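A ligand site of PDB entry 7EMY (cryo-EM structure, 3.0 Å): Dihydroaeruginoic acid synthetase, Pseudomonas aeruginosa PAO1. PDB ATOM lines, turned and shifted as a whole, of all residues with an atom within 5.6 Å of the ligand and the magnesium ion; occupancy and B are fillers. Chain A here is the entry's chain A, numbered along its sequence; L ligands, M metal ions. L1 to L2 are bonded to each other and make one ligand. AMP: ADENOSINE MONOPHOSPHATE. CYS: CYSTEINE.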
ATOM      1  N   THR A 697     -31.690  15.631  22.352  1.00  0.00           N
ATOM      2  CA  THR A 697     -30.482  16.401  22.558  1.00  0.00           C
ATOM      3  C   THR A 697     -29.609  15.742  23.620  1.00  0.00           C
ATOM      4  O   THR A 697     -30.085  15.115  24.560  1.00  0.00           O
ATOM      5  CB  THR A 697     -30.797  17.862  22.950  1.00  0.00           C
ATOM      6  OG1 THR A 697     -29.612  18.485  23.325  1.00  0.00           O
ATOM      7  CG2 THR A 697     -31.687  18.119  24.147  1.00  0.00           C
ATOM      8  N   PHE A 741     -31.240  13.919  14.388  1.00  0.00           N
ATOM      9  CA  PHE A 741     -30.916  15.321  14.176  1.00  0.00           C
ATOM     10  C   PHE A 741     -32.084  15.930  13.406  1.00  0.00           C
ATOM     11  O   PHE A 741     -32.398  15.497  12.292  1.00  0.00           O
ATOM     12  CB  PHE A 741     -29.577  15.396  13.441  1.00  0.00           C
ATOM     13  CG  PHE A 741     -28.847  16.722  13.498  1.00  0.00           C
ATOM     14  CD1 PHE A 741     -28.547  17.317  14.733  1.00  0.00           C
ATOM     15  CD2 PHE A 741     -28.369  17.311  12.311  1.00  0.00           C
ATOM     16  CE1 PHE A 741     -27.795  18.493  14.796  1.00  0.00           C
ATOM     17  CE2 PHE A 741     -27.596  18.485  12.378  1.00  0.00           C
ATOM     18  CZ  PHE A 741     -27.310  19.080  13.614  1.00  0.00           C
ATOM     19  N   ASP A 742     -32.789  16.900  13.978  1.00  0.00           N
ATOM     20  CA  ASP A 742     -34.130  17.224  13.500  1.00  0.00           C
ATOM     21  C   ASP A 742     -34.180  17.929  12.134  1.00  0.00           C
ATOM     22  O   ASP A 742     -35.242  18.013  11.545  1.00  0.00           O
ATOM     23  CB  ASP A 742     -34.974  17.944  14.554  1.00  0.00           C
ATOM     24  CG  ASP A 742     -34.503  19.319  14.974  1.00  0.00           C
ATOM     25  OD1 ASP A 742     -33.528  19.810  14.376  1.00  0.00           O
ATOM     26  OD2 ASP A 742     -35.095  19.832  15.939  1.00  0.00           O
ATOM     27  N   LEU A 743     -33.047  18.264  11.539  1.00  0.00           N
ATOM     28  CA  LEU A 743     -32.980  18.553  10.110  1.00  0.00           C
ATOM     29  C   LEU A 743     -33.635  17.451   9.276  1.00  0.00           C
ATOM     30  O   LEU A 743     -34.306  17.726   8.283  1.00  0.00           O
ATOM     31  CB  LEU A 743     -31.526  18.657   9.686  1.00  0.00           C
ATOM     32  CG  LEU A 743     -30.675  19.654  10.471  1.00  0.00           C
ATOM     33  CD1 LEU A 743     -29.352  19.839   9.740  1.00  0.00           C
ATOM     34  CD2 LEU A 743     -31.348  20.999  10.596  1.00  0.00           C
ATOM     35  N   LEU A 812     -28.245  24.963   5.187  1.00  0.00           N
ATOM     36  CA  LEU A 812     -27.165  24.692   6.127  1.00  0.00           C
ATOM     37  C   LEU A 812     -27.518  25.284   7.465  1.00  0.00           C
ATOM     38  O   LEU A 812     -27.991  26.404   7.533  1.00  0.00           O
ATOM     39  CB  LEU A 812     -25.846  25.272   5.655  1.00  0.00           C
ATOM     40  CG  LEU A 812     -25.406  24.768   4.283  1.00  0.00           C
ATOM     41  CD1 LEU A 812     -24.098  25.451   3.916  1.00  0.00           C
ATOM     42  CD2 LEU A 812     -25.206  23.262   4.268  1.00  0.00           C
ATOM     43  N   SER A 813     -27.323  24.555   8.543  1.00  0.00           N
ATOM     44  CA  SER A 813     -27.957  24.964   9.784  1.00  0.00           C
ATOM     45  C   SER A 813     -27.465  24.202  10.979  1.00  0.00           C
ATOM     46  O   SER A 813     -26.802  23.190  10.846  1.00  0.00           O
ATOM     47  CB  SER A 813     -29.432  24.684   9.625  1.00  0.00           C
ATOM     48  OG  SER A 813     -29.595  23.319   9.327  1.00  0.00           O
ATOM     49  N   GLY A 814     -27.792  24.640  12.183  1.00  0.00           N
ATOM     50  CA  GLY A 814     -27.507  23.832  13.349  1.00  0.00           C
ATOM     51  C   GLY A 814     -26.033  23.754  13.691  1.00  0.00           C
ATOM     52  O   GLY A 814     -25.694  22.998  14.592  1.00  0.00           O
ATOM     53  N   ASP A 815     -25.162  24.480  13.009  1.00  0.00           N
ATOM     54  CA  ASP A 815     -23.764  24.712  13.319  1.00  0.00           C
ATOM     55  C   ASP A 815     -23.276  25.922  12.499  1.00  0.00           C
ATOM     56  O   ASP A 815     -23.917  26.263  11.512  1.00  0.00           O
ATOM     57  CB  ASP A 815     -22.921  23.487  12.977  1.00  0.00           C
ATOM     58  CG  ASP A 815     -21.464  23.613  13.446  1.00  0.00           C
ATOM     59  OD1 ASP A 815     -21.221  24.405  14.374  1.00  0.00           O
ATOM     60  OD2 ASP A 815     -20.590  22.915  12.884  1.00  0.00           O
ATOM     61  N   TRP A 816     -22.149  26.520  12.855  1.00  0.00           N
ATOM     62  CA  TRP A 816     -21.577  27.665  12.139  1.00  0.00           C
ATOM     63  C   TRP A 816     -21.321  27.381  10.665  1.00  0.00           C
ATOM     64  O   TRP A 816     -20.480  26.556  10.317  1.00  0.00           O
ATOM     65  CB  TRP A 816     -20.242  28.017  12.774  1.00  0.00           C
ATOM     66  CG  TRP A 816     -20.309  28.624  14.119  1.00  0.00           C
ATOM     67  CD1 TRP A 816     -19.811  28.090  15.248  1.00  0.00           C
ATOM     68  CD2 TRP A 816     -20.796  29.949  14.460  1.00  0.00           C
ATOM     69  NE1 TRP A 816     -19.905  29.018  16.265  1.00  0.00           N
ATOM     70  CE2 TRP A 816     -20.435  30.201  15.810  1.00  0.00           C
ATOM     71  CE3 TRP A 816     -21.456  30.964  13.760  1.00  0.00           C
ATOM     72  CZ2 TRP A 816     -20.621  31.460  16.396  1.00  0.00           C
ATOM     73  CZ3 TRP A 816     -21.709  32.201  14.362  1.00  0.00           C
ATOM     74  CH2 TRP A 816     -21.262  32.460  15.661  1.00  0.00           C
ATOM     75  N   VAL A 817     -21.992  28.117   9.787  1.00  0.00           N
ATOM     76  CA  VAL A 817     -21.684  28.126   8.362  1.00  0.00           C
ATOM     77  C   VAL A 817     -20.558  29.113   8.139  1.00  0.00           C
ATOM     78  O   VAL A 817     -20.705  30.295   8.402  1.00  0.00           O
ATOM     79  CB  VAL A 817     -22.931  28.501   7.539  1.00  0.00           C
ATOM     80  CG1 VAL A 817     -22.679  28.256   6.054  1.00  0.00           C
ATOM     81  CG2 VAL A 817     -24.149  27.666   7.940  1.00  0.00           C
ATOM     82  N   VAL A 837     -28.983  29.713   5.006  1.00  0.00           N
ATOM     83  CA  VAL A 837     -28.417  29.350   6.286  1.00  0.00           C
ATOM     84  C   VAL A 837     -29.477  29.528   7.325  1.00  0.00           C
ATOM     85  O   VAL A 837     -30.111  30.566   7.370  1.00  0.00           O
ATOM     86  CB  VAL A 837     -27.182  30.181   6.592  1.00  0.00           C
ATOM     87  CG1 VAL A 837     -26.704  29.963   8.021  1.00  0.00           C
ATOM     88  CG2 VAL A 837     -26.101  29.800   5.572  1.00  0.00           C
ATOM     89  N   LEU A 838     -29.710  28.530   8.165  1.00  0.00           N
ATOM     90  CA  LEU A 838     -30.834  28.533   9.082  1.00  0.00           C
ATOM     91  C   LEU A 838     -30.389  28.352  10.504  1.00  0.00           C
ATOM     92  O   LEU A 838     -29.442  27.646  10.807  1.00  0.00           O
ATOM     93  CB  LEU A 838     -31.891  27.513   8.693  1.00  0.00           C
ATOM     94  CG  LEU A 838     -32.422  27.710   7.278  1.00  0.00           C
ATOM     95  CD1 LEU A 838     -31.683  26.814   6.295  1.00  0.00           C
ATOM     96  CD2 LEU A 838     -33.891  27.334   7.213  1.00  0.00           C
ATOM     97  N   GLY A 839     -31.087  29.045  11.381  1.00  0.00           N
ATOM     98  CA  GLY A 839     -30.726  29.177  12.764  1.00  0.00           C
ATOM     99  C   GLY A 839     -31.673  28.435  13.685  1.00  0.00           C
ATOM    100  O   GLY A 839     -32.673  27.872  13.228  1.00  0.00           O
ATOM    101  N   GLY A 840     -31.418  28.512  14.977  1.00  0.00           N
ATOM    102  CA  GLY A 840     -32.343  28.053  16.003  1.00  0.00           C
ATOM    103  C   GLY A 840     -32.160  26.596  16.341  1.00  0.00           C
ATOM    104  O   GLY A 840     -31.701  25.812  15.539  1.00  0.00           O
ATOM    105  N   ALA A 841     -32.467  26.264  17.587  1.00  0.00           N
ATOM    106  CA  ALA A 841     -32.100  24.977  18.145  1.00  0.00           C
ATOM    107  C   ALA A 841     -33.134  23.899  17.842  1.00  0.00           C
ATOM    108  O   ALA A 841     -34.246  24.209  17.422  1.00  0.00           O
ATOM    109  CB  ALA A 841     -31.940  25.136  19.659  1.00  0.00           C
ATOM    110  N   THR A 842     -32.824  22.657  18.207  1.00  0.00           N
ATOM    111  CA  THR A 842     -33.747  21.537  18.244  1.00  0.00           C
ATOM    112  C   THR A 842     -35.118  21.913  18.835  1.00  0.00           C
ATOM    113  O   THR A 842     -36.177  21.559  18.345  1.00  0.00           O
ATOM    114  CB  THR A 842     -33.183  20.437  19.142  1.00  0.00           C
ATOM    115  OG1 THR A 842     -31.773  20.266  19.082  1.00  0.00           O
ATOM    116  CG2 THR A 842     -33.828  19.075  18.881  1.00  0.00           C
ATOM    117  N   GLU A 843     -35.114  22.696  19.896  1.00  0.00           N
ATOM    118  CA  GLU A 843     -36.258  23.123  20.678  1.00  0.00           C
ATOM    119  C   GLU A 843     -37.203  24.100  20.015  1.00  0.00           C
ATOM    120  O   GLU A 843     -38.244  24.424  20.570  1.00  0.00           O
ATOM    121  CB  GLU A 843     -35.733  23.701  21.977  1.00  0.00           C
ATOM    122  CG  GLU A 843     -35.094  22.637  22.874  1.00  0.00           C
ATOM    123  CD  GLU A 843     -33.577  22.531  22.740  1.00  0.00           C
ATOM    124  OE1 GLU A 843     -33.022  22.710  21.645  1.00  0.00           O
ATOM    125  OE2 GLU A 843     -32.899  22.306  23.766  1.00  0.00           O
ATOM    126  N   ILE A 846     -37.443  22.829  14.017  1.00  0.00           N
ATOM    127  CA  ILE A 846     -36.211  22.394  13.361  1.00  0.00           C
ATOM    128  C   ILE A 846     -35.296  23.595  13.321  1.00  0.00           C
ATOM    129  O   ILE A 846     -34.204  23.601  13.871  1.00  0.00           O
ATOM    130  CB  ILE A 846     -36.452  21.832  11.940  1.00  0.00           C
ATOM    131  CG1 ILE A 846     -37.445  20.662  11.833  1.00  0.00           C
ATOM    132  CG2 ILE A 846     -35.125  21.380  11.341  1.00  0.00           C
ATOM    133  CD1 ILE A 846     -38.900  21.110  11.626  1.00  0.00           C
ATOM    134  N   TRP A 847     -35.814  24.683  12.724  1.00  0.00           N
ATOM    135  CA  TRP A 847     -35.140  25.946  12.515  1.00  0.00           C
ATOM    136  C   TRP A 847     -36.049  27.087  12.840  1.00  0.00           C
ATOM    137  O   TRP A 847     -37.272  26.970  12.812  1.00  0.00           O
ATOM    138  CB  TRP A 847     -34.828  26.166  11.055  1.00  0.00           C
ATOM    139  CG  TRP A 847     -34.041  25.129  10.402  1.00  0.00           C
ATOM    140  CD1 TRP A 847     -32.743  24.866  10.636  1.00  0.00           C
ATOM    141  CD2 TRP A 847     -34.487  24.187   9.406  1.00  0.00           C
ATOM    142  NE1 TRP A 847     -32.346  23.885   9.773  1.00  0.00           N
ATOM    143  CE2 TRP A 847     -33.359  23.461   8.971  1.00  0.00           C
ATOM    144  CE3 TRP A 847     -35.718  23.903   8.797  1.00  0.00           C
ATOM    145  CZ2 TRP A 847     -33.427  22.545   7.923  1.00  0.00           C
ATOM    146  CZ3 TRP A 847     -35.817  22.932   7.806  1.00  0.00           C
ATOM    147  CH2 TRP A 847     -34.664  22.283   7.335  1.00  0.00           C
ATOM    148  N   ILE A 863     -21.922  34.077   9.225  1.00  0.00           N
ATOM    149  CA  ILE A 863     -23.206  34.178   8.530  1.00  0.00           C
ATOM    150  C   ILE A 863     -24.282  34.338   9.603  1.00  0.00           C
ATOM    151  O   ILE A 863     -24.417  33.445  10.440  1.00  0.00           O
ATOM    152  CB  ILE A 863     -23.489  33.008   7.586  1.00  0.00           C
ATOM    153  CG1 ILE A 863     -22.388  32.963   6.513  1.00  0.00           C
ATOM    154  CG2 ILE A 863     -24.877  33.195   6.980  1.00  0.00           C
ATOM    155  CD1 ILE A 863     -22.575  31.931   5.400  1.00  0.00           C
ATOM    156  N   TYR A 865     -27.876  34.673  11.780  1.00  0.00           N
ATOM    157  CA  TYR A 865     -29.267  34.298  11.653  1.00  0.00           C
ATOM    158  C   TYR A 865     -29.972  35.435  10.913  1.00  0.00           C
ATOM    159  O   TYR A 865     -29.823  36.609  11.249  1.00  0.00           O
ATOM    160  CB  TYR A 865     -29.900  34.094  13.023  1.00  0.00           C
ATOM    161  CG  TYR A 865     -29.500  32.916  13.868  1.00  0.00           C
ATOM    162  CD1 TYR A 865     -28.540  31.974  13.469  1.00  0.00           C
ATOM    163  CD2 TYR A 865     -30.154  32.761  15.105  1.00  0.00           C
ATOM    164  CE1 TYR A 865     -28.256  30.877  14.304  1.00  0.00           C
ATOM    165  CE2 TYR A 865     -29.886  31.661  15.925  1.00  0.00           C
ATOM    166  CZ  TYR A 865     -28.934  30.721  15.521  1.00  0.00           C
ATOM    167  OH  TYR A 865     -28.732  29.622  16.272  1.00  0.00           O
ATOM    168  N   TYR A 874     -37.609  35.803  17.234  1.00  0.00           N
ATOM    169  CA  TYR A 874     -36.463  35.872  18.092  1.00  0.00           C
ATOM    170  C   TYR A 874     -36.506  37.084  18.984  1.00  0.00           C
ATOM    171  O   TYR A 874     -36.761  38.206  18.570  1.00  0.00           O
ATOM    172  CB  TYR A 874     -35.192  35.903  17.288  1.00  0.00           C
ATOM    173  CG  TYR A 874     -34.649  34.547  17.091  1.00  0.00           C
ATOM    174  CD1 TYR A 874     -35.200  33.739  16.095  1.00  0.00           C
ATOM    175  CD2 TYR A 874     -33.636  34.082  17.924  1.00  0.00           C
ATOM    176  CE1 TYR A 874     -34.659  32.478  15.891  1.00  0.00           C
ATOM    177  CE2 TYR A 874     -33.066  32.832  17.681  1.00  0.00           C
ATOM    178  CZ  TYR A 874     -33.565  32.042  16.653  1.00  0.00           C
ATOM    179  OH  TYR A 874     -32.986  30.873  16.362  1.00  0.00           O
ATOM    180  N   ILE A 894     -36.066  32.129  21.213  1.00  0.00           N
ATOM    181  CA  ILE A 894     -36.912  31.773  20.078  1.00  0.00           C
ATOM    182  C   ILE A 894     -38.338  31.656  20.548  1.00  0.00           C
ATOM    183  O   ILE A 894     -38.549  31.167  21.645  1.00  0.00           O
ATOM    184  CB  ILE A 894     -36.529  30.453  19.426  1.00  0.00           C
ATOM    185  CG1 ILE A 894     -35.017  30.334  19.295  1.00  0.00           C
ATOM    186  CG2 ILE A 894     -37.222  30.388  18.071  1.00  0.00           C
ATOM    187  CD1 ILE A 894     -34.488  29.091  18.610  1.00  0.00           C
ATOM    188  N   THR A 925     -32.666  29.948  24.543  1.00  0.00           N
ATOM    189  CA  THR A 925     -31.666  29.034  23.967  1.00  0.00           C
ATOM    190  C   THR A 925     -30.336  28.932  24.686  1.00  0.00           C
ATOM    191  O   THR A 925     -29.681  27.914  24.543  1.00  0.00           O
ATOM    192  CB  THR A 925     -31.288  29.443  22.539  1.00  0.00           C
ATOM    193  OG1 THR A 925     -30.678  30.682  22.604  1.00  0.00           O
ATOM    194  CG2 THR A 925     -32.384  29.611  21.515  1.00  0.00           C
ATOM    195  N   ASP A 927     -27.960  30.502  23.323  1.00  0.00           N
ATOM    196  CA  ASP A 927     -27.216  31.150  22.251  1.00  0.00           C
ATOM    197  C   ASP A 927     -27.016  32.607  22.631  1.00  0.00           C
ATOM    198  O   ASP A 927     -27.933  33.261  23.105  1.00  0.00           O
ATOM    199  CB  ASP A 927     -27.934  31.120  20.894  1.00  0.00           C
ATOM    200  CG  ASP A 927     -27.936  29.820  20.100  1.00  0.00           C
ATOM    201  OD1 ASP A 927     -27.324  28.818  20.540  1.00  0.00           O
ATOM    202  OD2 ASP A 927     -28.504  29.814  18.981  1.00  0.00           O
ATOM    203  N   PHE A 939     -26.062  35.695  15.302  1.00  0.00           N
ATOM    204  CA  PHE A 939     -25.719  34.684  16.277  1.00  0.00           C
ATOM    205  C   PHE A 939     -24.223  34.786  16.581  1.00  0.00           C
ATOM    206  O   PHE A 939     -23.403  35.001  15.686  1.00  0.00           O
ATOM    207  CB  PHE A 939     -26.121  33.325  15.724  1.00  0.00           C
ATOM    208  CG  PHE A 939     -25.562  32.162  16.484  1.00  0.00           C
ATOM    209  CD1 PHE A 939     -25.997  31.906  17.792  1.00  0.00           C
ATOM    210  CD2 PHE A 939     -24.544  31.385  15.928  1.00  0.00           C
ATOM    211  CE1 PHE A 939     -25.402  30.863  18.521  1.00  0.00           C
ATOM    212  CE2 PHE A 939     -23.955  30.346  16.668  1.00  0.00           C
ATOM    213  CZ  PHE A 939     -24.420  30.059  17.949  1.00  0.00           C
ATOM    214  N   ARG A 942     -22.004  30.552  21.895  1.00  0.00           N
ATOM    215  CA  ARG A 942     -22.605  30.184  23.172  1.00  0.00           C
ATOM    216  C   ARG A 942     -21.671  30.482  24.334  1.00  0.00           C
ATOM    217  O   ARG A 942     -20.463  30.337  24.217  1.00  0.00           O
ATOM    218  CB  ARG A 942     -22.997  28.710  23.132  1.00  0.00           C
ATOM    219  CG  ARG A 942     -24.021  28.444  22.011  1.00  0.00           C
ATOM    220  CD  ARG A 942     -24.727  27.110  22.139  1.00  0.00           C
ATOM    221  NE  ARG A 942     -25.368  26.985  23.447  1.00  0.00           N
ATOM    222  CZ  ARG A 942     -26.635  27.080  23.742  1.00  0.00           C
ATOM    223  NH1 ARG A 942     -27.549  27.352  22.871  1.00  0.00           N
ATOM    224  NH2 ARG A 942     -27.060  26.896  24.957  1.00  0.00           N
ATOM    225  N   GLN A 946     -23.120  23.792  25.859  1.00  0.00           N
ATOM    226  CA  GLN A 946     -23.627  23.238  24.601  1.00  0.00           C
ATOM    227  C   GLN A 946     -22.704  23.656  23.480  1.00  0.00           C
ATOM    228  O   GLN A 946     -22.508  24.841  23.223  1.00  0.00           O
ATOM    229  CB  GLN A 946     -25.074  23.680  24.341  1.00  0.00           C
ATOM    230  CG  GLN A 946     -25.631  23.259  22.960  1.00  0.00           C
ATOM    231  CD  GLN A 946     -27.116  23.553  22.742  1.00  0.00           C
ATOM    232  OE1 GLN A 946     -27.655  23.394  21.635  1.00  0.00           O
ATOM    233  NE2 GLN A 946     -27.867  23.961  23.728  1.00  0.00           N
ATOM    234  N   LYS A 948     -20.775  22.196  19.465  1.00  0.00           N
ATOM    235  CA  LYS A 948     -20.978  21.470  18.225  1.00  0.00           C
ATOM    236  C   LYS A 948     -19.762  20.590  17.977  1.00  0.00           C
ATOM    237  O   LYS A 948     -18.635  21.075  18.014  1.00  0.00           O
ATOM    238  CB  LYS A 948     -21.175  22.483  17.104  1.00  0.00           C
ATOM    239  CG  LYS A 948     -22.406  23.395  17.315  1.00  0.00           C
ATOM    240  CD  LYS A 948     -23.669  22.858  16.667  1.00  0.00           C
ATOM    241  CE  LYS A 948     -24.438  21.793  17.459  1.00  0.00           C
ATOM    242  NZ  LYS A 948     -25.558  21.263  16.636  1.00  0.00           N
ATOM    243  N   GLY A 951     -20.735  19.047  13.580  1.00  0.00           N
ATOM    244  CA  GLY A 951     -22.018  19.751  13.391  1.00  0.00           C
ATOM    245  C   GLY A 951     -23.143  19.308  14.315  1.00  0.00           C
ATOM    246  O   GLY A 951     -24.053  20.089  14.595  1.00  0.00           O
ATOM    247  N   ARG A 953     -24.893  18.105  18.037  1.00  0.00           N
ATOM    248  CA  ARG A 953     -24.996  18.846  19.298  1.00  0.00           C
ATOM    249  C   ARG A 953     -24.573  17.990  20.455  1.00  0.00           C
ATOM    250  O   ARG A 953     -25.121  16.896  20.651  1.00  0.00           O
ATOM    251  CB  ARG A 953     -26.455  19.251  19.491  1.00  0.00           C
ATOM    252  CG  ARG A 953     -26.716  20.038  20.787  1.00  0.00           C
ATOM    253  CD  ARG A 953     -28.224  19.998  21.003  1.00  0.00           C
ATOM    254  NE  ARG A 953     -28.630  20.786  22.163  1.00  0.00           N
ATOM    255  CZ  ARG A 953     -29.807  21.359  22.331  1.00  0.00           C
ATOM    256  NH1 ARG A 953     -30.651  21.492  21.341  1.00  0.00           N
ATOM    257  NH2 ARG A 953     -30.160  21.852  23.471  1.00  0.00           N
ATOM    258  N   GLU A 955     -23.609  18.466  24.790  1.00  0.00           N
ATOM    259  CA  GLU A 955     -23.461  19.306  25.962  1.00  0.00           C
ATOM    260  C   GLU A 955     -22.235  18.780  26.685  1.00  0.00           C
ATOM    261  O   GLU A 955     -22.153  17.598  26.992  1.00  0.00           O
ATOM    262  CB  GLU A 955     -24.704  19.258  26.865  1.00  0.00           C
ATOM    263  CG  GLU A 955     -26.073  19.349  26.163  1.00  0.00           C
ATOM    264  CD  GLU A 955     -26.605  20.736  25.792  1.00  0.00           C
ATOM    265  OE1 GLU A 955     -26.578  21.630  26.666  1.00  0.00           O
ATOM    266  OE2 GLU A 955     -27.126  20.895  24.663  1.00  0.00           O
HETATM  267  P   AMP L   1     -28.776  22.465  17.653  1.00  0.00           P
HETATM  268  O1P AMP L   1     -28.715  21.171  16.958  1.00  0.00           O
HETATM  269  O2P AMP L   1     -30.052  22.670  18.356  1.00  0.00           O
HETATM  270  O3P AMP L   1     -27.830  22.273  18.780  1.00  0.00           O
HETATM  271  O5' AMP L   1     -28.347  23.717  16.793  1.00  0.00           O
HETATM  272  C5' AMP L   1     -27.052  24.237  17.006  1.00  0.00           C
HETATM  273  C4' AMP L   1     -26.919  25.141  18.271  1.00  0.00           C
HETATM  274  O4' AMP L   1     -26.366  26.373  17.816  1.00  0.00           O
HETATM  275  C3' AMP L   1     -28.208  25.607  18.952  1.00  0.00           C
HETATM  276  O3' AMP L   1     -27.873  26.270  20.168  1.00  0.00           O
HETATM  277  C2' AMP L   1     -28.720  26.580  17.913  1.00  0.00           C
HETATM  278  O2' AMP L   1     -29.605  27.565  18.427  1.00  0.00           O
HETATM  279  C1' AMP L   1     -27.431  27.138  17.248  1.00  0.00           C
HETATM  280  N9  AMP L   1     -27.394  27.010  15.790  1.00  0.00           N
HETATM  281  C8  AMP L   1     -28.457  26.686  14.945  1.00  0.00           C
HETATM  282  N7  AMP L   1     -28.234  27.044  13.670  1.00  0.00           N
HETATM  283  C5  AMP L   1     -26.993  27.570  13.741  1.00  0.00           C
HETATM  284  C6  AMP L   1     -26.267  28.209  12.748  1.00  0.00           C
HETATM  285  N6  AMP L   1     -26.741  28.423  11.519  1.00  0.00           N
HETATM  286  N1  AMP L   1     -25.085  28.725  12.962  1.00  0.00           N
HETATM  287  C2  AMP L   1     -24.586  28.521  14.175  1.00  0.00           C
HETATM  288  N3  AMP L   1     -25.211  27.921  15.205  1.00  0.00           N
HETATM  289  C4  AMP L   1     -26.449  27.520  14.964  1.00  0.00           C
HETATM  290  N   CYS L   2     -30.025  20.568  13.822  1.00  0.00           N
HETATM  291  CA  CYS L   2     -29.907  21.558  14.925  1.00  0.00           C
HETATM  292  C   CYS L   2     -29.778  20.966  16.378  1.00  0.00           C
HETATM  293  O   CYS L   2     -30.582  20.134  16.773  1.00  0.00           O
HETATM  294  CB  CYS L   2     -31.022  22.601  14.894  1.00  0.00           C
HETATM  295  SG  CYS L   2     -30.905  23.702  13.433  1.00  0.00           S
HETATM  296 MG    MG M   1     -29.264  22.211  19.911  1.00  0.00          MG
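An oxygen (O2') of AMP L1 lies close to the side-chain carboxylate (OD2) of Asp 927 (2.6 Å). The backbone NH of Thr 842 sits close to an oxygen (O2P) of AMP L1 (2.8 Å). An oxygen (O2P) of AMP L1 lies close to the side-chain hydroxyl (OG1) of Thr 842, 3.0 Å away. O3P of AMP L1 sits close to OE1 of Gln 946, 3.1 Å away. A nitrogen (N7) of AMP L1 sits close to the backbone NH (N) of Gly 814. O of Leu 838 sits close to N6 of AMP L1 (2.9 Å). An oxygen (O3') of AMP L1 lies close to the guanidinium group (NH1) of Arg 942 (2.9 Å). OH of Tyr 865 sits close to N9 of AMP L1, at 3.0 Å. O of Gly 840 sits close to SG of CYS L2, at 3.1 Å. The backbone carbonyl oxygen (O) of Asp 815 lies close to a nitrogen (N1) of AMP L1, at 3.1 Å. O2' of AMP L1 sits close to N of Ala 841 (3.3 Å). The side-chain amino group of Lys 948 sits close to an oxygen (O3P) of AMP L1, at 3.3 Å. SG of CYS L2 sits close to O of Ile 846 (3.3 Å).
The guanidinium group of Arg 953 sits close to the side-chain hydroxyl of Thr 842. OD1 of Asp 927 is in salt-bridge range of NH1 of Arg 942, 2.8 Å away. The side-chain carboxylate of Asp 927 lies within hydrogen-bond range of the side-chain hydroxyl of Tyr 865, at 2.7 Å. The backbone NH (N) of Asp 927 sits at hydrogen-bond distance from the side-chain hydroxyl (OG1) of Thr 925, at 2.8 Å. The side-chain carboxylate (OE2) of Glu 955 sits close to the side-chain amide nitrogen (NE2) of Gln 946, 3.3 Å away. The backbone carbonyl oxygen of Gly 814 lies within hydrogen-bond range of the side-chain amino group of Lys 948, at 2.7 Å. The backbone carbonyl oxygen (O) of Thr 925 is in hydrogen-bond range of the guanidinium group (NH1) of Arg 942 (2.8 Å). OH of Tyr 865 lies within hydrogen-bond range of N of Gly 840 (3.2 Å).
Residues that only touch the ligand: Phe 939, Phe 741, Gly 839, Trp 816, Leu 743, Trp 847, Asp 742, Val 837 and Ser 813. Hydrophobic or aromatic side chains within 4 Å of the ligand: Phe 741, Leu 743, Trp 816, Val 837, Ala 841, Trp 847, Tyr 865 and Phe 939.
Residues that only touch the magnesium ion: Thr 842 (3.3 Å) and Ala 841 (3.97 Å). The nearest printed residue that does not touch the magnesium ion is Glu 843 (4.2 Å).
The magnesium ion is bound by O2P of AMP L1 (1.8 Å), O3P of AMP L1 (1.8 Å) and NH1 of Arg 953 (2.1 Å). The magnesium ion has three donor atoms within binding distance. Slightly farther from the magnesium ion lies the side-chain amide oxygen (OE1) of Gln 946 (2.6 Å). Slightly farther from the magnesium ion lies the guanidinium group (NE) of Arg 953 (2.7 Å).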
